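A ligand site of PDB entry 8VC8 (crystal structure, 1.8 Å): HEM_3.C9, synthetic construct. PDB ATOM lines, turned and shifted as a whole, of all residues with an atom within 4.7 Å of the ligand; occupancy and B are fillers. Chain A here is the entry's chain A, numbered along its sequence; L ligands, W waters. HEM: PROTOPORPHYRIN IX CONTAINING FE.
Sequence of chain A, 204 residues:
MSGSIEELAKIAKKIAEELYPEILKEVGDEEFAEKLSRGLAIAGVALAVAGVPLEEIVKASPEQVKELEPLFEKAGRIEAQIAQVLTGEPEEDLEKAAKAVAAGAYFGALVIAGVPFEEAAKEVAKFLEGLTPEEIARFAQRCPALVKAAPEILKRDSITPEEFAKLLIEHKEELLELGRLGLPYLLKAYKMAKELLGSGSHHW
The side-chain sulfur (SG) of Cys 143 binds an iron atom (FE) of the ligand.
The guanidinium group of Arg 38 lies within salt-bridge range of an oxygen (O2A) of the ligand, 2.5 Å away.
The guanidinium group of Arg 142 lies within salt-bridge range of an oxygen (O2D) of the ligand, 2.9 Å away.
SG of Cys 143 sits close to N of Ala 145 (3.4 Å).
N of Leu 146 lies close to SG of Cys 143, at 3.3 Å.
The side-chain hydroxyl (OG1) of Thr 87 sits at hydrogen-bond distance from the backbone carbonyl oxygen (O) of Ala 83 (2.8 Å).
O of Lys 35 touches CMA of the ligand (3.2 Å).
Leu 36 touches the ligand.
CA of Gly 39 touches CMA of the ligand (3.7 Å).
Ala 83 touches the ligand.
CB of Pro 90 touches O2D of the ligand (3.99 Å).
O of Ala 100 touches CBC of the ligand, at 2.9 Å.
CG1 of Val 101 touches C2D of the ligand (3.3 Å).
Ala 103 touches the ligand (CB to CBC, 3.8 Å).
Gly 104 touches the ligand (CA to C2C, 3.7 Å).
Phe 139 touches the ligand.
Pro 144 touches the ligand.
Ala 145 touches the ligand (CB to C2B, 3.3 Å).
Leu 146 touches the ligand.
CZ of Phe 164 touches CAC of the ligand (3.7 Å).
Leu 175 touches the ligand (O to CBB, 3.98 Å).
Hydrophobic or aromatic side chains that line the ligand: Leu 36, Ala 83, Pro 90, Ala 100, Val 101, Ala 103, Pro 144, Ala 145, Leu 146 and Phe 164.
Of the 25 residues printed, 18 come within 4 Å of the ligand.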
ATOM      1  N   LYS A  35     -11.258  29.302 -19.026  1.00  0.00           N
ATOM      2  CA  LYS A  35     -11.899  28.022 -18.728  1.00  0.00           C
ATOM      3  C   LYS A  35     -12.196  27.242 -20.009  1.00  0.00           C
ATOM      4  O   LYS A  35     -11.971  26.029 -20.078  1.00  0.00           O
ATOM      5  CB  LYS A  35     -13.186  28.283 -17.959  1.00  0.00           C
ATOM      6  CG  LYS A  35     -12.978  28.715 -16.484  1.00  0.00           C
ATOM      7  CD  LYS A  35     -14.345  28.942 -15.839  1.00  0.00           C
ATOM      8  CE  LYS A  35     -14.283  29.597 -14.455  1.00  0.00           C
ATOM      9  NZ  LYS A  35     -15.688  29.850 -13.934  1.00  0.00           N
ATOM     10  N   LEU A  36     -12.785  27.904 -21.020  1.00  0.00           N
ATOM     11  CA  LEU A  36     -13.050  27.211 -22.285  1.00  0.00           C
ATOM     12  C   LEU A  36     -11.782  26.620 -22.896  1.00  0.00           C
ATOM     13  O   LEU A  36     -11.809  25.516 -23.463  1.00  0.00           O
ATOM     14  CB  LEU A  36     -13.643  28.197 -23.310  1.00  0.00           C
ATOM     15  CG  LEU A  36     -15.120  28.427 -23.286  1.00  0.00           C
ATOM     16  CD1 LEU A  36     -15.393  29.500 -24.370  1.00  0.00           C
ATOM     17  CD2 LEU A  36     -15.876  27.072 -23.572  1.00  0.00           C
ATOM     18  N   ARG A  38      -8.992  25.618 -21.429  1.00  0.00           N
ATOM     19  CA  ARG A  38      -8.542  24.410 -20.708  1.00  0.00           C
ATOM     20  C   ARG A  38      -9.497  23.230 -20.947  1.00  0.00           C
ATOM     21  O   ARG A  38      -9.072  22.095 -21.155  1.00  0.00           O
ATOM     22  CB  ARG A  38      -8.456  24.727 -19.203  1.00  0.00           C
ATOM     23  CG  ARG A  38      -8.052  23.579 -18.281  1.00  0.00           C
ATOM     24  CD  ARG A  38      -7.882  24.094 -16.848  1.00  0.00           C
ATOM     25  NE  ARG A  38      -9.130  24.673 -16.332  1.00  0.00           N
ATOM     26  CZ  ARG A  38      -9.187  25.625 -15.422  1.00  0.00           C
ATOM     27  NH1 ARG A  38      -8.100  26.115 -14.862  1.00  0.00           N
ATOM     28  NH2 ARG A  38     -10.379  26.101 -15.049  1.00  0.00           N
ATOM     29  N   GLY A  39     -10.807  23.480 -20.830  1.00  0.00           N
ATOM     30  CA  GLY A  39     -11.777  22.386 -20.957  1.00  0.00           C
ATOM     31  C   GLY A  39     -11.768  21.786 -22.362  1.00  0.00           C
ATOM     32  O   GLY A  39     -11.840  20.565 -22.508  1.00  0.00           O
ATOM     33  N   LEU A  40     -11.695  22.629 -23.389  1.00  0.00           N
ATOM     34  CA  LEU A  40     -11.678  22.098 -24.765  1.00  0.00           C
ATOM     35  C   LEU A  40     -10.384  21.323 -25.055  1.00  0.00           C
ATOM     36  O   LEU A  40     -10.412  20.310 -25.738  1.00  0.00           O
ATOM     37  CB  LEU A  40     -11.852  23.226 -25.774  1.00  0.00           C
ATOM     38  CG  LEU A  40     -13.256  23.811 -25.664  1.00  0.00           C
ATOM     39  CD1 LEU A  40     -13.337  25.113 -26.473  1.00  0.00           C
ATOM     40  CD2 LEU A  40     -14.359  22.785 -26.111  1.00  0.00           C
ATOM     41  N   ALA A  80     -11.882  13.597 -16.340  1.00  0.00           N
ATOM     42  CA  ALA A  80     -11.947  13.962 -14.932  1.00  0.00           C
ATOM     43  C   ALA A  80     -10.605  13.746 -14.247  1.00  0.00           C
ATOM     44  O   ALA A  80     -10.251  14.499 -13.320  1.00  0.00           O
ATOM     45  CB  ALA A  80     -13.059  13.173 -14.245  1.00  0.00           C
ATOM     46  N   ALA A  83      -8.417  16.673 -15.282  1.00  0.00           N
ATOM     47  CA  ALA A  83      -8.901  17.880 -14.621  1.00  0.00           C
ATOM     48  C   ALA A  83      -8.418  17.958 -13.184  1.00  0.00           C
ATOM     49  O   ALA A  83      -8.149  19.055 -12.678  1.00  0.00           O
ATOM     50  CB  ALA A  83     -10.421  17.971 -14.673  1.00  0.00           C
ATOM     51  N   THR A  87      -6.543  21.381 -12.318  1.00  0.00           N
ATOM     52  CA  THR A  87      -7.304  22.248 -11.437  1.00  0.00           C
ATOM     53  C   THR A  87      -7.315  21.833  -9.967  1.00  0.00           C
ATOM     54  O   THR A  87      -7.589  22.672  -9.110  1.00  0.00           O
ATOM     55  CB  THR A  87      -8.764  22.314 -11.912  1.00  0.00           C
ATOM     56  OG1 THR A  87      -9.455  21.167 -11.389  1.00  0.00           O
ATOM     57  CG2 THR A  87      -8.845  22.280 -13.427  1.00  0.00           C
ATOM     58  N   PRO A  90     -11.767  18.540  -8.893  1.00  0.00           N
ATOM     59  CA  PRO A  90     -12.529  17.278  -8.940  1.00  0.00           C
ATOM     60  C   PRO A  90     -11.903  16.173  -8.115  1.00  0.00           C
ATOM     61  O   PRO A  90     -11.633  15.086  -8.648  1.00  0.00           O
ATOM     62  CB  PRO A  90     -12.533  16.934 -10.442  1.00  0.00           C
ATOM     63  CG  PRO A  90     -11.339  17.610 -10.968  1.00  0.00           C
ATOM     64  CD  PRO A  90     -11.214  18.873 -10.218  1.00  0.00           C
ATOM     65  N   ALA A 100     -20.875  12.191 -15.494  1.00  0.00           N
ATOM     66  CA  ALA A 100     -21.472  13.470 -15.808  1.00  0.00           C
ATOM     67  C   ALA A 100     -20.799  14.128 -16.999  1.00  0.00           C
ATOM     68  O   ALA A 100     -21.483  14.552 -17.946  1.00  0.00           O
ATOM     69  CB  ALA A 100     -21.430  14.404 -14.589  1.00  0.00           C
ATOM     70  N   VAL A 101     -19.463  14.243 -16.976  1.00  0.00           N
ATOM     71  CA  VAL A 101     -18.750  14.911 -18.068  1.00  0.00           C
ATOM     72  C   VAL A 101     -18.868  14.102 -19.335  1.00  0.00           C
ATOM     73  O   VAL A 101     -18.896  14.688 -20.423  1.00  0.00           O
ATOM     74  CB  VAL A 101     -17.235  15.169 -17.806  1.00  0.00           C
ATOM     75  CG1 VAL A 101     -16.993  16.515 -17.287  1.00  0.00           C
ATOM     76  CG2 VAL A 101     -16.622  14.150 -16.965  1.00  0.00           C
ATOM     77  N   ALA A 103     -21.433  12.678 -20.352  1.00  0.00           N
ATOM     78  CA  ALA A 103     -22.710  13.081 -20.953  1.00  0.00           C
ATOM     79  C   ALA A 103     -22.557  14.289 -21.875  1.00  0.00           C
ATOM     80  O   ALA A 103     -23.198  14.351 -22.927  1.00  0.00           O
ATOM     81  CB  ALA A 103     -23.726  13.396 -19.854  1.00  0.00           C
ATOM     82  N   GLY A 104     -21.700  15.243 -21.519  1.00  0.00           N
ATOM     83  CA  GLY A 104     -21.443  16.384 -22.366  1.00  0.00           C
ATOM     84  C   GLY A 104     -21.046  16.089 -23.810  1.00  0.00           C
ATOM     85  O   GLY A 104     -21.693  16.565 -24.750  1.00  0.00           O
ATOM     86  N   PHE A 107     -23.821  14.005 -25.687  1.00  0.00           N
ATOM     87  CA  PHE A 107     -24.905  14.893 -26.137  1.00  0.00           C
ATOM     88  C   PHE A 107     -24.536  15.644 -27.399  1.00  0.00           C
ATOM     89  O   PHE A 107     -25.265  15.626 -28.421  1.00  0.00           O
ATOM     90  CB  PHE A 107     -25.221  15.878 -25.011  1.00  0.00           C
ATOM     91  CG  PHE A 107     -26.326  16.832 -25.326  1.00  0.00           C
ATOM     92  CD1 PHE A 107     -27.592  16.371 -25.562  1.00  0.00           C
ATOM     93  CD2 PHE A 107     -26.106  18.186 -25.317  1.00  0.00           C
ATOM     94  CE1 PHE A 107     -28.625  17.257 -25.827  1.00  0.00           C
ATOM     95  CE2 PHE A 107     -27.128  19.073 -25.592  1.00  0.00           C
ATOM     96  CZ  PHE A 107     -28.405  18.587 -25.853  1.00  0.00           C
ATOM     97  N   PHE A 139     -22.638  18.589 -10.035  1.00  0.00           N
ATOM     98  CA  PHE A 139     -21.757  18.531 -11.206  1.00  0.00           C
ATOM     99  C   PHE A 139     -22.147  19.563 -12.244  1.00  0.00           C
ATOM    100  O   PHE A 139     -21.272  20.111 -12.919  1.00  0.00           O
ATOM    101  CB  PHE A 139     -21.797  17.155 -11.866  1.00  0.00           C
ATOM    102  CG  PHE A 139     -21.260  16.038 -10.974  1.00  0.00           C
ATOM    103  CD1 PHE A 139     -20.124  16.216 -10.199  1.00  0.00           C
ATOM    104  CD2 PHE A 139     -21.911  14.804 -10.936  1.00  0.00           C
ATOM    105  CE1 PHE A 139     -19.642  15.191  -9.364  1.00  0.00           C
ATOM    106  CE2 PHE A 139     -21.442  13.768 -10.128  1.00  0.00           C
ATOM    107  CZ  PHE A 139     -20.312  13.969  -9.326  1.00  0.00           C
ATOM    108  N   ARG A 142     -20.498  22.800 -11.823  1.00  0.00           N
ATOM    109  CA  ARG A 142     -19.089  22.902 -12.198  1.00  0.00           C
ATOM    110  C   ARG A 142     -18.852  23.188 -13.668  1.00  0.00           C
ATOM    111  O   ARG A 142     -17.692  23.397 -14.071  1.00  0.00           O
ATOM    112  CB  ARG A 142     -18.350  21.618 -11.844  1.00  0.00           C
ATOM    113  CG  ARG A 142     -18.358  21.284 -10.371  1.00  0.00           C
ATOM    114  CD  ARG A 142     -17.152  20.426 -10.089  1.00  0.00           C
ATOM    115  NE  ARG A 142     -17.381  19.462  -9.029  1.00  0.00           N
ATOM    116  CZ  ARG A 142     -16.796  18.265  -8.983  1.00  0.00           C
ATOM    117  NH1 ARG A 142     -15.963  17.875  -9.944  1.00  0.00           N
ATOM    118  NH2 ARG A 142     -17.071  17.445  -7.976  1.00  0.00           N
ATOM    119  N   CYS A 143     -19.883  23.154 -14.518  1.00  0.00           N
ATOM    120  CA  CYS A 143     -19.698  23.464 -15.936  1.00  0.00           C
ATOM    121  C   CYS A 143     -19.936  24.950 -16.185  1.00  0.00           C
ATOM    122  O   CYS A 143     -21.077  25.442 -15.996  1.00  0.00           O
ATOM    123  CB  CYS A 143     -20.656  22.642 -16.779  1.00  0.00           C
ATOM    124  SG  CYS A 143     -20.537  23.086 -18.486  1.00  0.00           S
ATOM    125  N   PRO A 144     -18.941  25.706 -16.667  1.00  0.00           N
ATOM    126  CA  PRO A 144     -19.190  27.137 -16.946  1.00  0.00           C
ATOM    127  C   PRO A 144     -20.068  27.384 -18.152  1.00  0.00           C
ATOM    128  O   PRO A 144     -20.678  28.444 -18.222  1.00  0.00           O
ATOM    129  CB  PRO A 144     -17.774  27.719 -17.142  1.00  0.00           C
ATOM    130  CG  PRO A 144     -16.932  26.565 -17.601  1.00  0.00           C
ATOM    131  CD  PRO A 144     -17.497  25.366 -16.796  1.00  0.00           C
ATOM    132  N   ALA A 145     -20.190  26.431 -19.080  1.00  0.00           N
ATOM    133  CA  ALA A 145     -21.139  26.624 -20.170  1.00  0.00           C
ATOM    134  C   ALA A 145     -22.559  26.428 -19.693  1.00  0.00           C
ATOM    135  O   ALA A 145     -23.423  27.254 -20.034  1.00  0.00           O
ATOM    136  CB  ALA A 145     -20.841  25.663 -21.313  1.00  0.00           C
ATOM    137  N   LEU A 146     -22.846  25.360 -18.934  1.00  0.00           N
ATOM    138  CA  LEU A 146     -24.201  25.220 -18.367  1.00  0.00           C
ATOM    139  C   LEU A 146     -24.563  26.400 -17.468  1.00  0.00           C
ATOM    140  O   LEU A 146     -25.714  26.851 -17.476  1.00  0.00           O
ATOM    141  CB  LEU A 146     -24.356  23.914 -17.566  1.00  0.00           C
ATOM    142  CG  LEU A 146     -24.181  22.615 -18.338  1.00  0.00           C
ATOM    143  CD1 LEU A 146     -24.206  21.423 -17.357  1.00  0.00           C
ATOM    144  CD2 LEU A 146     -25.228  22.513 -19.428  1.00  0.00           C
ATOM    145  N   PHE A 164     -32.934  17.688 -15.688  1.00  0.00           N
ATOM    146  CA  PHE A 164     -31.722  18.136 -16.373  1.00  0.00           C
ATOM    147  C   PHE A 164     -31.989  18.247 -17.873  1.00  0.00           C
ATOM    148  O   PHE A 164     -31.636  19.247 -18.495  1.00  0.00           O
ATOM    149  CB  PHE A 164     -30.574  17.160 -16.077  1.00  0.00           C
ATOM    150  CG  PHE A 164     -29.233  17.630 -16.637  1.00  0.00           C
ATOM    151  CD1 PHE A 164     -28.502  18.569 -15.925  1.00  0.00           C
ATOM    152  CD2 PHE A 164     -28.789  17.207 -17.833  1.00  0.00           C
ATOM    153  CE1 PHE A 164     -27.268  19.072 -16.441  1.00  0.00           C
ATOM    154  CE2 PHE A 164     -27.563  17.671 -18.373  1.00  0.00           C
ATOM    155  CZ  PHE A 164     -26.804  18.606 -17.683  1.00  0.00           C
ATOM    156  N   LEU A 168     -31.745  21.677 -20.468  1.00  0.00           N
ATOM    157  CA  LEU A 168     -31.093  21.741 -21.782  1.00  0.00           C
ATOM    158  C   LEU A 168     -32.063  22.266 -22.831  1.00  0.00           C
ATOM    159  O   LEU A 168     -31.724  23.177 -23.608  1.00  0.00           O
ATOM    160  CB  LEU A 168     -30.553  20.352 -22.173  1.00  0.00           C
ATOM    161  CG  LEU A 168     -29.472  19.660 -21.298  1.00  0.00           C
ATOM    162  CD1 LEU A 168     -29.097  18.253 -21.852  1.00  0.00           C
ATOM    163  CD2 LEU A 168     -28.210  20.536 -21.098  1.00  0.00           C
ATOM    164  N   LEU A 175     -27.256  27.024 -25.651  1.00  0.00           N
ATOM    165  CA  LEU A 175     -26.350  25.888 -25.643  1.00  0.00           C
ATOM    166  C   LEU A 175     -25.874  25.540 -27.048  1.00  0.00           C
ATOM    167  O   LEU A 175     -24.710  25.155 -27.218  1.00  0.00           O
ATOM    168  CB  LEU A 175     -26.996  24.673 -24.993  1.00  0.00           C
ATOM    169  CG  LEU A 175     -27.225  24.783 -23.484  1.00  0.00           C
ATOM    170  CD1 LEU A 175     -28.172  23.678 -23.047  1.00  0.00           C
ATOM    171  CD2 LEU A 175     -25.863  24.673 -22.709  1.00  0.00           C
ATOM    172  N   LEU A 178     -23.019  28.092 -27.754  1.00  0.00           N
ATOM    173  CA  LEU A 178     -21.763  27.712 -27.100  1.00  0.00           C
ATOM    174  C   LEU A 178     -21.130  26.477 -27.748  1.00  0.00           C
ATOM    175  O   LEU A 178     -19.917  26.408 -27.907  1.00  0.00           O
ATOM    176  CB  LEU A 178     -21.996  27.449 -25.612  1.00  0.00           C
ATOM    177  CG  LEU A 178     -22.383  28.707 -24.847  1.00  0.00           C
ATOM    178  CD1 LEU A 178     -22.930  28.393 -23.397  1.00  0.00           C
ATOM    179  CD2 LEU A 178     -21.234  29.682 -24.738  1.00  0.00           C
ATOM    180  N   GLY A 179     -21.935  25.458 -28.065  1.00  0.00           N
ATOM    181  CA  GLY A 179     -21.376  24.314 -28.752  1.00  0.00           C
ATOM    182  C   GLY A 179     -20.817  24.672 -30.130  1.00  0.00           C
ATOM    183  O   GLY A 179     -19.793  24.123 -30.540  1.00  0.00           O
HETATM  184  CHA HEM L   1     -16.704  21.186 -17.326  1.00  0.00           C
HETATM  185  CHB HEM L   1     -17.472  23.491 -21.531  1.00  0.00           C
HETATM  186  CHC HEM L   1     -21.780  21.230 -22.122  1.00  0.00           C
HETATM  187  CHD HEM L   1     -20.855  18.707 -18.038  1.00  0.00           C
HETATM  188  C1A HEM L   1     -16.557  21.964 -18.428  1.00  0.00           C
HETATM  189  C2A HEM L   1     -15.428  22.834 -18.652  1.00  0.00           C
HETATM  190  C3A HEM L   1     -15.671  23.479 -19.811  1.00  0.00           C
HETATM  191  C4A HEM L   1     -16.944  23.041 -20.359  1.00  0.00           C
HETATM  192  CMA HEM L   1     -14.727  24.495 -20.507  1.00  0.00           C
HETATM  193  CAA HEM L   1     -14.162  22.913 -17.735  1.00  0.00           C
HETATM  194  CBA HEM L   1     -14.184  24.130 -16.857  1.00  0.00           C
HETATM  195  CGA HEM L   1     -12.812  24.427 -16.251  1.00  0.00           C
HETATM  196  O1A HEM L   1     -11.784  23.797 -16.603  1.00  0.00           O
HETATM  197  O2A HEM L   1     -12.775  25.341 -15.400  1.00  0.00           O
HETATM  198  C1B HEM L   1     -18.696  23.065 -22.043  1.00  0.00           C
HETATM  199  C2B HEM L   1     -19.296  23.546 -23.281  1.00  0.00           C
HETATM  200  C3B HEM L   1     -20.452  22.934 -23.425  1.00  0.00           C
HETATM  201  C4B HEM L   1     -20.680  22.045 -22.332  1.00  0.00           C
HETATM  202  CMB HEM L   1     -18.783  24.582 -24.336  1.00  0.00           C
HETATM  203  CAB HEM L   1     -21.347  23.257 -24.650  1.00  0.00           C
HETATM  204  CBB HEM L   1     -22.628  22.930 -24.652  1.00  0.00           C
HETATM  205  C1C HEM L   1     -21.893  20.339 -21.061  1.00  0.00           C
HETATM  206  C2C HEM L   1     -22.941  19.367 -20.867  1.00  0.00           C
HETATM  207  C3C HEM L   1     -22.686  18.682 -19.775  1.00  0.00           C
HETATM  208  C4C HEM L   1     -21.446  19.152 -19.207  1.00  0.00           C
HETATM  209  CMC HEM L   1     -24.216  19.117 -21.732  1.00  0.00           C
HETATM  210  CAC HEM L   1     -23.621  17.568 -19.305  1.00  0.00           C
HETATM  211  CBC HEM L   1     -23.301  16.812 -18.265  1.00  0.00           C
HETATM  212  C1D HEM L   1     -19.691  19.237 -17.514  1.00  0.00           C
HETATM  213  C2D HEM L   1     -19.105  18.850 -16.247  1.00  0.00           C
HETATM  214  C3D HEM L   1     -17.974  19.525 -16.070  1.00  0.00           C
HETATM  215  C4D HEM L   1     -17.800  20.356 -17.209  1.00  0.00           C
HETATM  216  CMD HEM L   1     -19.588  17.821 -15.180  1.00  0.00           C
HETATM  217  CAD HEM L   1     -17.082  19.365 -14.805  1.00  0.00           C
HETATM  218  CBD HEM L   1     -15.727  18.752 -15.122  1.00  0.00           C
HETATM  219  CGD HEM L   1     -15.037  18.095 -13.956  1.00  0.00           C
HETATM  220  O1D HEM L   1     -14.055  17.326 -14.219  1.00  0.00           O
HETATM  221  O2D HEM L   1     -15.459  18.318 -12.783  1.00  0.00           O
HETATM  222  NA  HEM L   1     -17.492  22.121 -19.466  1.00  0.00           N
HETATM  223  NB  HEM L   1     -19.556  22.108 -21.449  1.00  0.00           N
HETATM  224  NC  HEM L   1     -20.965  20.151 -20.036  1.00  0.00           N
HETATM  225  ND  HEM L   1     -18.875  20.236 -18.121  1.00  0.00           N
HETATM  226 FE   HEM L   1     -19.371  21.339 -19.585  1.00  0.00          FE
HETATM  227  O   HOH W   1     -22.555  20.413 -26.598  1.00  0.00           O
